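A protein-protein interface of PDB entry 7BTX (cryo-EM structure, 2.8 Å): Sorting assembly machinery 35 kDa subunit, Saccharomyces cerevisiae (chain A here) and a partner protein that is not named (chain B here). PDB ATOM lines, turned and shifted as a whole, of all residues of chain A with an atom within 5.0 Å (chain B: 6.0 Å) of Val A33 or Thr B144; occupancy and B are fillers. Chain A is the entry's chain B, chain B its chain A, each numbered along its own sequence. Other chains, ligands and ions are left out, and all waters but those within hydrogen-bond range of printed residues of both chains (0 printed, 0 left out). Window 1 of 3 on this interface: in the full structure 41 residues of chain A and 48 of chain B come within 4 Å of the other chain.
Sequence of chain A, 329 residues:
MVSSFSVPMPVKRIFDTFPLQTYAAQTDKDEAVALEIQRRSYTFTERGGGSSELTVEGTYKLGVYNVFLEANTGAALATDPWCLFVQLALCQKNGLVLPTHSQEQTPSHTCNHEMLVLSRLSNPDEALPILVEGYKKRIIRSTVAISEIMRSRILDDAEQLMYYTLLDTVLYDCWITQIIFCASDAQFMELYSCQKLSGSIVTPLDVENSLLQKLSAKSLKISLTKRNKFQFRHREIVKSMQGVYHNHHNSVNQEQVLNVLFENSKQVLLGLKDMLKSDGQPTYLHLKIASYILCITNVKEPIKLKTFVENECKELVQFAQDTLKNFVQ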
ATOM      1  N   ASP A  30       9.541   7.632 -13.716  1.00  0.00           N
ATOM      2  CA  ASP A  30       8.842   8.154 -14.881  1.00  0.00           C
ATOM      3  C   ASP A  30       9.815   8.189 -16.050  1.00  0.00           C
ATOM      4  O   ASP A  30      10.788   8.948 -16.032  1.00  0.00           O
ATOM      5  CB  ASP A  30       8.285   9.545 -14.591  1.00  0.00           C
ATOM      6  CG  ASP A  30       7.293  10.006 -15.636  1.00  0.00           C
ATOM      7  OD1 ASP A  30       6.912   9.198 -16.505  1.00  0.00           O
ATOM      8  OD2 ASP A  30       6.887  11.183 -15.588  1.00  0.00           O
ATOM      9  N   GLU A  31       9.562   7.361 -17.056  1.00  0.00           N
ATOM     10  CA  GLU A  31      10.448   7.268 -18.202  1.00  0.00           C
ATOM     11  C   GLU A  31      10.294   8.456 -19.139  1.00  0.00           C
ATOM     12  O   GLU A  31      11.222   8.763 -19.890  1.00  0.00           O
ATOM     13  CB  GLU A  31      10.186   5.948 -18.945  1.00  0.00           C
ATOM     14  CG  GLU A  31      11.224   5.553 -19.988  1.00  0.00           C
ATOM     15  CD  GLU A  31      10.739   5.746 -21.409  1.00  0.00           C
ATOM     16  OE1 GLU A  31       9.586   6.183 -21.592  1.00  0.00           O
ATOM     17  OE2 GLU A  31      11.514   5.457 -22.346  1.00  0.00           O
ATOM     18  N   ALA A  32       9.165   9.160 -19.076  1.00  0.00           N
ATOM     19  CA  ALA A  32       8.993  10.354 -19.889  1.00  0.00           C
ATOM     20  C   ALA A  32       9.796  11.524 -19.343  1.00  0.00           C
ATOM     21  O   ALA A  32      10.171  12.420 -20.103  1.00  0.00           O
ATOM     22  CB  ALA A  32       7.515  10.714 -19.978  1.00  0.00           C
ATOM     23  N   VAL A  33      10.072  11.534 -18.038  1.00  0.00           N
ATOM     24  CA  VAL A  33      10.918  12.571 -17.456  1.00  0.00           C
ATOM     25  C   VAL A  33      12.378  12.322 -17.812  1.00  0.00           C
ATOM     26  O   VAL A  33      13.112  13.253 -18.157  1.00  0.00           O
ATOM     27  CB  VAL A  33      10.684  12.643 -15.934  1.00  0.00           C
ATOM     28  CG1 VAL A  33      11.811  13.353 -15.217  1.00  0.00           C
ATOM     29  CG2 VAL A  33       9.391  13.359 -15.652  1.00  0.00           C
ATOM     30  N   ALA A  34      12.805  11.058 -17.794  1.00  0.00           N
ATOM     31  CA  ALA A  34      14.174  10.710 -18.149  1.00  0.00           C
ATOM     32  C   ALA A  34      14.475  10.930 -19.625  1.00  0.00           C
ATOM     33  O   ALA A  34      15.645  11.061 -19.990  1.00  0.00           O
ATOM     34  CB  ALA A  34      14.458   9.255 -17.784  1.00  0.00           C
ATOM     35  N   LEU A  35      13.457  10.968 -20.479  1.00  0.00           N
ATOM     36  CA  LEU A  35      13.660  11.317 -21.876  1.00  0.00           C
ATOM     37  C   LEU A  35      13.770  12.819 -22.076  1.00  0.00           C
ATOM     38  O   LEU A  35      14.460  13.264 -22.996  1.00  0.00           O
ATOM     39  CB  LEU A  35      12.522  10.768 -22.737  1.00  0.00           C
ATOM     40  CG  LEU A  35      12.433   9.263 -22.948  1.00  0.00           C
ATOM     41  CD1 LEU A  35      11.252   8.948 -23.827  1.00  0.00           C
ATOM     42  CD2 LEU A  35      13.701   8.728 -23.557  1.00  0.00           C
ATOM     43  N   GLU A  36      13.096  13.613 -21.241  1.00  0.00           N
ATOM     44  CA  GLU A  36      13.234  15.061 -21.334  1.00  0.00           C
ATOM     45  C   GLU A  36      14.593  15.513 -20.824  1.00  0.00           C
ATOM     46  O   GLU A  36      15.201  16.428 -21.388  1.00  0.00           O
ATOM     47  CB  GLU A  36      12.136  15.760 -20.542  1.00  0.00           C
ATOM     48  CG  GLU A  36      12.031  17.241 -20.845  1.00  0.00           C
ATOM     49  CD  GLU A  36      11.099  17.973 -19.905  1.00  0.00           C
ATOM     50  OE1 GLU A  36      10.718  17.394 -18.871  1.00  0.00           O
ATOM     51  OE2 GLU A  36      10.720  19.121 -20.212  1.00  0.00           O
ATOM     52  N   ILE A  37      15.067  14.903 -19.735  1.00  0.00           N
ATOM     53  CA  ILE A  37      16.368  15.237 -19.171  1.00  0.00           C
ATOM     54  C   ILE A  37      17.480  14.857 -20.134  1.00  0.00           C
ATOM     55  O   ILE A  37      18.449  15.604 -20.299  1.00  0.00           O
ATOM     56  CB  ILE A  37      16.526  14.551 -17.799  1.00  0.00           C
ATOM     57  CG1 ILE A  37      15.521  15.125 -16.804  1.00  0.00           C
ATOM     58  CG2 ILE A  37      17.922  14.717 -17.242  1.00  0.00           C
ATOM     59  CD1 ILE A  37      15.471  14.386 -15.506  1.00  0.00           C
ATOM     60  N   SER B 142      16.774  17.820  -7.254  1.00  0.00           N
ATOM     61  CA  SER B 142      16.963  16.639  -8.070  1.00  0.00           C
ATOM     62  C   SER B 142      16.782  16.989  -9.538  1.00  0.00           C
ATOM     63  O   SER B 142      16.207  18.020  -9.885  1.00  0.00           O
ATOM     64  CB  SER B 142      15.971  15.559  -7.671  1.00  0.00           C
ATOM     65  OG  SER B 142      14.661  16.080  -7.666  1.00  0.00           O
ATOM     66  N   GLY B 143      17.273  16.102 -10.406  1.00  0.00           N
ATOM     67  CA  GLY B 143      17.174  16.337 -11.836  1.00  0.00           C
ATOM     68  C   GLY B 143      15.749  16.353 -12.345  1.00  0.00           C
ATOM     69  O   GLY B 143      15.454  17.005 -13.345  1.00  0.00           O
ATOM     70  N   THR B 144      14.847  15.659 -11.661  1.00  0.00           N
ATOM     71  CA  THR B 144      13.438  15.698 -12.002  1.00  0.00           C
ATOM     72  C   THR B 144      12.729  16.927 -11.462  1.00  0.00           C
ATOM     73  O   THR B 144      11.555  17.115 -11.768  1.00  0.00           O
ATOM     74  CB  THR B 144      12.729  14.453 -11.476  1.00  0.00           C
ATOM     75  OG1 THR B 144      11.395  14.410 -11.988  1.00  0.00           O
ATOM     76  CG2 THR B 144      12.637  14.525  -9.993  1.00  0.00           C
ATOM     77  N   MET B 145      13.377  17.743 -10.641  1.00  0.00           N
ATOM     78  CA  MET B 145      12.785  19.004 -10.223  1.00  0.00           C
ATOM     79  C   MET B 145      13.351  20.181 -10.984  1.00  0.00           C
ATOM     80  O   MET B 145      12.637  21.157 -11.220  1.00  0.00           O
ATOM     81  CB  MET B 145      12.991  19.228  -8.724  1.00  0.00           C
ATOM     82  CG  MET B 145      11.980  18.527  -7.857  1.00  0.00           C
ATOM     83  SD  MET B 145      10.300  19.089  -8.135  1.00  0.00           S
ATOM     84  CE  MET B 145       9.419  18.016  -7.013  1.00  0.00           C
ATOM     85  N   LEU B 146      14.620  20.098 -11.376  1.00  0.00           N
ATOM     86  CA  LEU B 146      15.210  21.102 -12.244  1.00  0.00           C
ATOM     87  C   LEU B 146      14.602  21.063 -13.634  1.00  0.00           C
ATOM     88  O   LEU B 146      14.536  22.096 -14.308  1.00  0.00           O
ATOM     89  CB  LEU B 146      16.715  20.889 -12.322  1.00  0.00           C
ATOM     90  CG  LEU B 146      17.457  20.895 -10.995  1.00  0.00           C
ATOM     91  CD1 LEU B 146      18.829  20.299 -11.170  1.00  0.00           C
ATOM     92  CD2 LEU B 146      17.540  22.298 -10.464  1.00  0.00           C
ATOM     93  N   SER B 147      14.155  19.892 -14.075  1.00  0.00           N
ATOM     94  CA  SER B 147      13.579  19.725 -15.400  1.00  0.00           C
ATOM     95  C   SER B 147      12.120  20.140 -15.472  1.00  0.00           C
ATOM     96  O   SER B 147      11.590  20.298 -16.574  1.00  0.00           O
ATOM     97  CB  SER B 147      13.717  18.271 -15.838  1.00  0.00           C
ATOM     98  OG  SER B 147      13.164  18.057 -17.119  1.00  0.00           O
ATOM     99  N   GLN B 148      11.458  20.314 -14.335  1.00  0.00           N
ATOM    100  CA  GLN B 148      10.048  20.668 -14.324  1.00  0.00           C
ATOM    101  C   GLN B 148       9.808  22.142 -14.070  1.00  0.00           C
ATOM    102  O   GLN B 148       8.683  22.608 -14.263  1.00  0.00           O
ATOM    103  CB  GLN B 148       9.297  19.852 -13.268  1.00  0.00           C
ATOM    104  CG  GLN B 148       9.271  18.372 -13.556  1.00  0.00           C
ATOM    105  CD  GLN B 148       8.034  17.928 -14.274  1.00  0.00           C
ATOM    106  OE1 GLN B 148       7.065  17.516 -13.649  1.00  0.00           O
ATOM    107  NE2 GLN B 148       8.060  17.993 -15.598  1.00  0.00           N
ATOM    108  N   GLN B 226       6.142   8.550 -25.458  1.00  0.00           N
ATOM    109  CA  GLN B 226       6.592   9.042 -24.157  1.00  0.00           C
ATOM    110  C   GLN B 226       7.388  10.338 -24.210  1.00  0.00           C
ATOM    111  O   GLN B 226       8.144  10.637 -23.283  1.00  0.00           O
ATOM    112  CB  GLN B 226       7.408   7.972 -23.433  1.00  0.00           C
ATOM    113  CG  GLN B 226       6.584   6.803 -22.935  1.00  0.00           C
ATOM    114  CD  GLN B 226       5.739   7.158 -21.735  1.00  0.00           C
ATOM    115  OE1 GLN B 226       4.617   7.639 -21.873  1.00  0.00           O
ATOM    116  NE2 GLN B 226       6.269   6.909 -20.546  1.00  0.00           N
ATOM    117  N   PRO B 229       6.565  14.787 -20.952  1.00  0.00           N
ATOM    118  CA  PRO B 229       6.192  14.222 -19.652  1.00  0.00           C
ATOM    119  C   PRO B 229       5.116  15.027 -18.940  1.00  0.00           C
ATOM    120  O   PRO B 229       4.951  16.227 -19.162  1.00  0.00           O
ATOM    121  CB  PRO B 229       7.505  14.261 -18.863  1.00  0.00           C
ATOM    122  CG  PRO B 229       8.271  15.335 -19.489  1.00  0.00           C
ATOM    123  CD  PRO B 229       7.942  15.308 -20.940  1.00  0.00           C
ATOM    124  N   VAL B 230       4.374  14.336 -18.080  1.00  0.00           N
ATOM    125  CA  VAL B 230       3.320  14.974 -17.307  1.00  0.00           C
ATOM    126  C   VAL B 230       3.945  15.759 -16.164  1.00  0.00           C
ATOM    127  O   VAL B 230       4.887  15.292 -15.511  1.00  0.00           O
ATOM    128  CB  VAL B 230       2.329  13.907 -16.809  1.00  0.00           C
ATOM    129  CG1 VAL B 230       1.190  14.517 -16.029  1.00  0.00           C
ATOM    130  CG2 VAL B 230       1.790  13.118 -17.984  1.00  0.00           C
ATOM    131  N   ILE B 232       4.663  17.713 -12.608  1.00  0.00           N
ATOM    132  CA  ILE B 232       4.644  17.276 -11.215  1.00  0.00           C
ATOM    133  C   ILE B 232       3.366  17.717 -10.510  1.00  0.00           C
ATOM    134  O   ILE B 232       2.879  17.031  -9.604  1.00  0.00           O
ATOM    135  CB  ILE B 232       5.929  17.793 -10.517  1.00  0.00           C
ATOM    136  CG1 ILE B 232       6.075  17.260  -9.098  1.00  0.00           C
ATOM    137  CG2 ILE B 232       6.036  19.309 -10.541  1.00  0.00           C
ATOM    138  CD1 ILE B 232       6.562  15.875  -9.059  1.00  0.00           C
ATOM    139  N   ASP B 256      13.355  10.849  -6.275  1.00  0.00           N
ATOM    140  CA  ASP B 256      14.573  10.957  -7.066  1.00  0.00           C
ATOM    141  C   ASP B 256      15.797  10.985  -6.165  1.00  0.00           C
ATOM    142  O   ASP B 256      16.655  10.099  -6.243  1.00  0.00           O
ATOM    143  CB  ASP B 256      14.552  12.190  -7.952  1.00  0.00           C
ATOM    144  CG  ASP B 256      15.465  12.052  -9.150  1.00  0.00           C
ATOM    145  OD1 ASP B 256      16.098  10.988  -9.293  1.00  0.00           O
ATOM    146  OD2 ASP B 256      15.558  12.998  -9.951  1.00  0.00           O
ATOM    147  N   ASP B 259      13.077  14.047  -3.271  1.00  0.00           N
ATOM    148  CA  ASP B 259      11.955  14.777  -3.826  1.00  0.00           C
ATOM    149  C   ASP B 259      10.876  13.796  -4.240  1.00  0.00           C
ATOM    150  O   ASP B 259      11.164  12.792  -4.891  1.00  0.00           O
ATOM    151  CB  ASP B 259      12.401  15.617  -5.021  1.00  0.00           C
ATOM    152  CG  ASP B 259      13.259  16.788  -4.615  1.00  0.00           C
ATOM    153  OD1 ASP B 259      12.965  17.414  -3.582  1.00  0.00           O
ATOM    154  OD2 ASP B 259      14.229  17.084  -5.326  1.00  0.00           O
ATOM    155  N   VAL B 261       8.594  12.572  -6.613  1.00  0.00           N
ATOM    156  CA  VAL B 261       8.387  12.706  -8.051  1.00  0.00           C
ATOM    157  C   VAL B 261       6.952  12.442  -8.468  1.00  0.00           C
ATOM    158  O   VAL B 261       6.635  12.554  -9.657  1.00  0.00           O
ATOM    159  CB  VAL B 261       9.335  11.766  -8.816  1.00  0.00           C
ATOM    160  CG1 VAL B 261      10.723  11.901  -8.281  1.00  0.00           C
ATOM    161  CG2 VAL B 261       8.882  10.331  -8.703  1.00  0.00           C
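Of the 14 printed residues of chain B, 5 touch a printed residue of chain A.
Printed residues of chain B that touch a printed residue of chain A: Gly B143, Thr B144, Ser B147, Gln B226 and Pro B229.
Hydrophobic or aromatic side chains of chain A within 4 Å of the printed part of chain B: Ala A32, Val A33, Leu A35 and Ile A37.
Along chain A the printed residues that touch a printed residue of chain B span positions 31 to 37.
Among the printed residues, 10 pairs touch across the chains.
The side-chain carboxylate (OD2) of Asp B256 lies within hydrogen-bond range of the backbone NH (N) of Thr B144, 3.2 Å away.
The side-chain carboxylate (OD1) of Asp A30 lies close to the backbone NH (N) of Ala A32 (3.4 Å).
OG of Ser B147 sits at hydrogen-bond distance from OE1 of Glu A36 (3.1 Å).
Among the printed residues, merely in contact across the chains: Glu A31 with Gln B226 (3.3 Å), Ala A32 with Gln B226 (3.4 Å), Ala A32 with Pro B229 (3.5 Å), Val A33 with Thr B144 (3.4 Å), Val A33 with Pro B229 (3.8 Å), Leu A35 with Gln B226 (3.6 Å), Glu A36 with Pro B229 (3.3 Å), Ile A37 with Gly B143 (3.4 Å) and Ile A37 with Ser B147 (3.8 Å).
Printed residues of chain B within 4 Å of Glu A31: Gln B226.
Printed residues of chain B within 4 Å of Val A33: Thr B144 and Pro B229.
Printed residues of chain B within 4 Å of Leu A35: Gln B226 (3.6 Å).
Printed residues of chain A within 4 Å of Gly B143: Ile A37.
Thr B144 touches one residue of chain A.
Of the printed residues of chain A, Ser B147 touches Glu A36 and Ile A37.
Printed residues of chain A within 4 Å of Gln B226: Glu A31, Ala A32 and Leu A35.
Asp B259 touches none of the printed residues of chain A.
The nearest residue of chain B that does not touch Val A33 is Gln B148 (4.8 Å).
The nearest residue of chain A that does not touch Thr B144 is Ile A37 (4.1 Å).
The nearest printed residue of chain B that does not touch Glu A31 is Pro B229 (6.4 Å).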
